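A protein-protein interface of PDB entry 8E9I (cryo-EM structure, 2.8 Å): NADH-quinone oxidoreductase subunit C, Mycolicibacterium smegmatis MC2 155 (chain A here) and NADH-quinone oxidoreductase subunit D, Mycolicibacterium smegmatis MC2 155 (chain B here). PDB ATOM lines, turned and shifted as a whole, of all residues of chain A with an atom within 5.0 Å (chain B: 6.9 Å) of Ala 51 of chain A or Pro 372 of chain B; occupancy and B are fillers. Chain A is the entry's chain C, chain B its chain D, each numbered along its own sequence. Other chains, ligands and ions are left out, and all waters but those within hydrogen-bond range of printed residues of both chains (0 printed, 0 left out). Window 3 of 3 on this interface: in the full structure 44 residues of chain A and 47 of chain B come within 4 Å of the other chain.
O of Glu 23 of chain A sits at hydrogen-bond distance from N of Leu 52 of chain A, 3.0 Å away. The backbone carbonyl oxygen of Ala 26 of chain A lies within hydrogen-bond range of the backbone NH of Val 50 of chain A, at 2.4 Å. O of Gly 373 of chain B is in hydrogen-bond range of N of Ser 392 of chain B (2.9 Å).
Among the printed residues, pairs that only touch across the chains: Leu 52 of chain A with Gln 374 of chain B, Tyr 90 of chain A with Gln 374 of chain B, Val 50 of chain A with Asp 393 of chain B, Tyr 90 of chain A with Pro 372 of chain B, Tyr 90 of chain A with Leu 119 of chain B, Leu 52 of chain A with Gly 373 of chain B and Ala 51 of chain A with Pro 372 of chain B.
Printed residues of chain A within 4 Å of Pro 372 of chain B: Ala 51 (3.9 Å) and Tyr 90 (3.5 Å). Printed residues of chain A within 4 Å of Gln 374 of chain B: Leu 52 (3.2 Å) and Tyr 90 (3.3 Å). Printed residues of chain A within 4 Å of Asp 393 of chain B: Val 50 (3.4 Å). Of the printed residues of chain B, Leu 52 of chain A touches Gly 373 (3.8 Å) and Gln 374 (3.2 Å). Printed residues of chain B within 4 Å of Val 50 of chain A: Asp 393 (3.4 Å). Of the printed residues of chain B, Tyr 90 of chain A touches Leu 119, Pro 372 and Gln 374. The nearest printed residue of chain A that does not touch Pro 372 of chain B is Val 50 of chain A (4.02 Å). The nearest printed residue of chain B that does not touch Tyr 90 of chain A is Gly 373 of chain B (4.1 Å).
Printed residues of chain A that touch a printed residue of chain B: Val 50, Ala 51, Leu 52 and Tyr 90. Hydrophobic or aromatic side chains of chain A within 4 Å of the printed part of chain B: Val 50, Leu 52 and Tyr 90. Among the printed residues, 7 pairs touch across the chains.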
ATOM      1  N   PRO A  22       1.877   3.381  -4.662  1.00  0.00           N
ATOM      2  CA  PRO A  22       1.848   2.809  -3.315  1.00  0.00           C
ATOM      3  C   PRO A  22       2.806   1.640  -3.177  1.00  0.00           C
ATOM      4  O   PRO A  22       3.330   1.099  -4.153  1.00  0.00           O
ATOM      5  CB  PRO A  22       0.397   2.351  -3.160  1.00  0.00           C
ATOM      6  CG  PRO A  22      -0.028   2.040  -4.543  1.00  0.00           C
ATOM      7  CD  PRO A  22       0.661   3.048  -5.421  1.00  0.00           C
ATOM      8  N   GLU A  23       3.036   1.259  -1.924  1.00  0.00           N
ATOM      9  CA  GLU A  23       3.794   0.055  -1.612  1.00  0.00           C
ATOM     10  C   GLU A  23       2.836  -1.128  -1.633  1.00  0.00           C
ATOM     11  O   GLU A  23       1.820  -1.124  -0.930  1.00  0.00           O
ATOM     12  CB  GLU A  23       4.473   0.192  -0.253  1.00  0.00           C
ATOM     13  N   ILE A  24       3.141  -2.133  -2.448  1.00  0.00           N
ATOM     14  CA  ILE A  24       2.327  -3.359  -2.489  1.00  0.00           C
ATOM     15  C   ILE A  24       3.050  -4.373  -1.611  1.00  0.00           C
ATOM     16  O   ILE A  24       4.130  -4.876  -1.924  1.00  0.00           O
ATOM     17  CB  ILE A  24       2.093  -3.864  -3.916  1.00  0.00           C
ATOM     18  CG1 ILE A  24       3.407  -3.966  -4.690  1.00  0.00           C
ATOM     19  CG2 ILE A  24       1.123  -2.954  -4.643  1.00  0.00           C
ATOM     20  CD1 ILE A  24       3.269  -4.717  -5.987  1.00  0.00           C
ATOM     21  N   ALA A  26       1.610  -7.255  -0.776  1.00  0.00           N
ATOM     22  CA  ALA A  26       1.220  -8.577  -1.241  1.00  0.00           C
ATOM     23  C   ALA A  26       0.338  -8.416  -2.467  1.00  0.00           C
ATOM     24  O   ALA A  26      -0.253  -7.359  -2.695  1.00  0.00           O
ATOM     25  CB  ALA A  26       0.486  -9.364  -0.151  1.00  0.00           C
ATOM     26  N   PRO A  49      -3.496  -6.439  -6.205  1.00  0.00           N
ATOM     27  CA  PRO A  49      -2.354  -6.053  -5.372  1.00  0.00           C
ATOM     28  C   PRO A  49      -2.822  -5.477  -4.046  1.00  0.00           C
ATOM     29  O   PRO A  49      -3.870  -4.835  -3.963  1.00  0.00           O
ATOM     30  CB  PRO A  49      -1.633  -5.004  -6.223  1.00  0.00           C
ATOM     31  CG  PRO A  49      -2.689  -4.436  -7.082  1.00  0.00           C
ATOM     32  CD  PRO A  49      -3.653  -5.545  -7.364  1.00  0.00           C
ATOM     33  N   VAL A  50      -2.031  -5.718  -3.003  1.00  0.00           N
ATOM     34  CA  VAL A  50      -2.362  -5.262  -1.654  1.00  0.00           C
ATOM     35  C   VAL A  50      -1.525  -4.013  -1.404  1.00  0.00           C
ATOM     36  O   VAL A  50      -0.388  -4.078  -0.936  1.00  0.00           O
ATOM     37  CB  VAL A  50      -2.113  -6.341  -0.606  1.00  0.00           C
ATOM     38  CG1 VAL A  50      -2.533  -5.846   0.760  1.00  0.00           C
ATOM     39  CG2 VAL A  50      -2.852  -7.610  -0.967  1.00  0.00           C
ATOM     40  N   ALA A  51      -2.113  -2.857  -1.694  1.00  0.00           N
ATOM     41  CA  ALA A  51      -1.410  -1.588  -1.576  1.00  0.00           C
ATOM     42  C   ALA A  51      -1.740  -0.917  -0.250  1.00  0.00           C
ATOM     43  O   ALA A  51      -2.914  -0.776   0.109  1.00  0.00           O
ATOM     44  CB  ALA A  51      -1.784  -0.670  -2.736  1.00  0.00           C
ATOM     45  N   LEU A  52      -0.708  -0.506   0.473  1.00  0.00           N
ATOM     46  CA  LEU A  52      -0.905   0.415   1.575  1.00  0.00           C
ATOM     47  C   LEU A  52      -1.251   1.793   1.012  1.00  0.00           C
ATOM     48  O   LEU A  52      -1.054   2.050  -0.176  1.00  0.00           O
ATOM     49  CB  LEU A  52       0.350   0.498   2.436  1.00  0.00           C
ATOM     50  CG  LEU A  52       0.706  -0.789   3.176  1.00  0.00           C
ATOM     51  CD1 LEU A  52       1.962  -0.590   4.011  1.00  0.00           C
ATOM     52  CD2 LEU A  52      -0.451  -1.260   4.046  1.00  0.00           C
ATOM     53  N   PRO A  53      -1.799   2.684   1.834  1.00  0.00           N
ATOM     54  CA  PRO A  53      -2.163   4.008   1.322  1.00  0.00           C
ATOM     55  C   PRO A  53      -0.954   4.738   0.762  1.00  0.00           C
ATOM     56  O   PRO A  53       0.143   4.681   1.318  1.00  0.00           O
ATOM     57  CB  PRO A  53      -2.733   4.717   2.552  1.00  0.00           C
ATOM     58  CG  PRO A  53      -3.157   3.621   3.461  1.00  0.00           C
ATOM     59  CD  PRO A  53      -2.159   2.531   3.251  1.00  0.00           C
ATOM     60  N   TYR A  90      -3.727   8.414   7.204  1.00  0.00           N
ATOM     61  CA  TYR A  90      -4.701   7.339   7.106  1.00  0.00           C
ATOM     62  C   TYR A  90      -5.456   7.235   8.419  1.00  0.00           C
ATOM     63  O   TYR A  90      -4.843   7.125   9.484  1.00  0.00           O
ATOM     64  CB  TYR A  90      -4.017   6.011   6.775  1.00  0.00           C
ATOM     65  CG  TYR A  90      -4.983   4.876   6.584  1.00  0.00           C
ATOM     66  CD1 TYR A  90      -5.838   4.851   5.498  1.00  0.00           C
ATOM     67  CD2 TYR A  90      -5.042   3.832   7.486  1.00  0.00           C
ATOM     68  CE1 TYR A  90      -6.725   3.819   5.319  1.00  0.00           C
ATOM     69  CE2 TYR A  90      -5.922   2.796   7.312  1.00  0.00           C
ATOM     70  CZ  TYR A  90      -6.764   2.794   6.230  1.00  0.00           C
ATOM     71  OH  TYR A  90      -7.646   1.760   6.053  1.00  0.00           O
ATOM     72  N   LEU B 119      -9.156   0.737  11.706  1.00  0.00           N
ATOM     73  CA  LEU B 119      -8.850   0.226  10.376  1.00  0.00           C
ATOM     74  C   LEU B 119     -10.110   0.120   9.532  1.00  0.00           C
ATOM     75  O   LEU B 119     -10.113   0.498   8.357  1.00  0.00           O
ATOM     76  CB  LEU B 119      -8.169  -1.132  10.481  1.00  0.00           C
ATOM     77  CG  LEU B 119      -6.750  -1.142  11.039  1.00  0.00           C
ATOM     78  CD1 LEU B 119      -6.270  -2.565  11.159  1.00  0.00           C
ATOM     79  CD2 LEU B 119      -5.810  -0.338  10.167  1.00  0.00           C
ATOM     80  N   VAL B 370     -10.472  -6.941   7.050  1.00  0.00           N
ATOM     81  CA  VAL B 370     -10.257  -5.524   7.321  1.00  0.00           C
ATOM     82  C   VAL B 370      -9.554  -4.917   6.115  1.00  0.00           C
ATOM     83  O   VAL B 370      -8.738  -5.597   5.487  1.00  0.00           O
ATOM     84  CB  VAL B 370      -9.425  -5.317   8.598  1.00  0.00           C
ATOM     85  CG1 VAL B 370      -9.188  -3.852   8.853  1.00  0.00           C
ATOM     86  CG2 VAL B 370     -10.126  -5.945   9.775  1.00  0.00           C
ATOM     87  N   PRO B 371      -9.843  -3.672   5.749  1.00  0.00           N
ATOM     88  CA  PRO B 371      -9.130  -3.050   4.638  1.00  0.00           C
ATOM     89  C   PRO B 371      -7.650  -2.945   4.946  1.00  0.00           C
ATOM     90  O   PRO B 371      -7.263  -2.773   6.109  1.00  0.00           O
ATOM     91  CB  PRO B 371      -9.778  -1.664   4.533  1.00  0.00           C
ATOM     92  CG  PRO B 371     -11.097  -1.820   5.155  1.00  0.00           C
ATOM     93  CD  PRO B 371     -10.909  -2.798   6.259  1.00  0.00           C
ATOM     94  N   PRO B 372      -6.788  -3.042   3.938  1.00  0.00           N
ATOM     95  CA  PRO B 372      -5.351  -2.971   4.210  1.00  0.00           C
ATOM     96  C   PRO B 372      -4.977  -1.618   4.786  1.00  0.00           C
ATOM     97  O   PRO B 372      -5.577  -0.597   4.453  1.00  0.00           O
ATOM     98  CB  PRO B 372      -4.720  -3.191   2.835  1.00  0.00           C
ATOM     99  CG  PRO B 372      -5.740  -2.707   1.888  1.00  0.00           C
ATOM    100  CD  PRO B 372      -7.069  -3.043   2.496  1.00  0.00           C
ATOM    101  N   GLY B 373      -3.986  -1.615   5.660  1.00  0.00           N
ATOM    102  CA  GLY B 373      -3.508  -0.363   6.207  1.00  0.00           C
ATOM    103  C   GLY B 373      -2.930  -0.543   7.588  1.00  0.00           C
ATOM    104  O   GLY B 373      -2.976  -1.618   8.177  1.00  0.00           O
ATOM    105  N   GLN B 374      -2.393   0.554   8.103  1.00  0.00           N
ATOM    106  CA  GLN B 374      -1.716   0.581   9.388  1.00  0.00           C
ATOM    107  C   GLN B 374      -2.439   1.560  10.290  1.00  0.00           C
ATOM    108  O   GLN B 374      -3.072   2.500   9.809  1.00  0.00           O
ATOM    109  CB  GLN B 374      -0.268   1.017   9.238  1.00  0.00           C
ATOM    110  CG  GLN B 374       0.475   0.283   8.159  1.00  0.00           C
ATOM    111  CD  GLN B 374       1.929   0.690   8.046  1.00  0.00           C
ATOM    112  OE1 GLN B 374       2.543   0.514   6.996  1.00  0.00           O
ATOM    113  NE2 GLN B 374       2.494   1.226   9.124  1.00  0.00           N
ATOM    114  N   VAL B 391      -1.579  -3.750  11.666  1.00  0.00           N
ATOM    115  CA  VAL B 391      -1.387  -3.746  10.225  1.00  0.00           C
ATOM    116  C   VAL B 391      -2.275  -4.822   9.631  1.00  0.00           C
ATOM    117  O   VAL B 391      -2.256  -5.970  10.090  1.00  0.00           O
ATOM    118  CB  VAL B 391       0.078  -3.993   9.833  1.00  0.00           C
ATOM    119  CG1 VAL B 391       0.256  -3.840   8.340  1.00  0.00           C
ATOM    120  CG2 VAL B 391       0.996  -3.059  10.587  1.00  0.00           C
ATOM    121  N   SER B 392      -3.040  -4.452   8.613  1.00  0.00           N
ATOM    122  CA  SER B 392      -3.938  -5.345   7.907  1.00  0.00           C
ATOM    123  C   SER B 392      -3.518  -5.436   6.450  1.00  0.00           C
ATOM    124  O   SER B 392      -3.165  -4.426   5.833  1.00  0.00           O
ATOM    125  CB  SER B 392      -5.377  -4.847   8.000  1.00  0.00           C
ATOM    126  OG  SER B 392      -6.233  -5.637   7.199  1.00  0.00           O
ATOM    127  N   ASP B 393      -3.552  -6.650   5.906  1.00  0.00           N
ATOM    128  CA  ASP B 393      -3.249  -6.892   4.503  1.00  0.00           C
ATOM    129  C   ASP B 393      -4.505  -7.171   3.691  1.00  0.00           C
ATOM    130  O   ASP B 393      -4.449  -7.878   2.680  1.00  0.00           O
ATOM    131  CB  ASP B 393      -2.266  -8.053   4.370  1.00  0.00           C
ATOM    132  N   GLY B 394      -5.644  -6.642   4.121  1.00  0.00           N
ATOM    133  CA  GLY B 394      -6.893  -6.904   3.446  1.00  0.00           C
ATOM    134  C   GLY B 394      -7.508  -8.245   3.765  1.00  0.00           C
ATOM    135  O   GLY B 394      -8.586  -8.553   3.244  1.00  0.00           O
ATOM    136  N   GLY B 395      -6.868  -9.051   4.610  1.00  0.00           N
ATOM    137  CA  GLY B 395      -7.327 -10.394   4.877  1.00  0.00           C
ATOM    138  C   GLY B 395      -8.124 -10.497   6.158  1.00  0.00           C
ATOM    139  O   GLY B 395      -8.298  -9.538   6.905  1.00  0.00           O
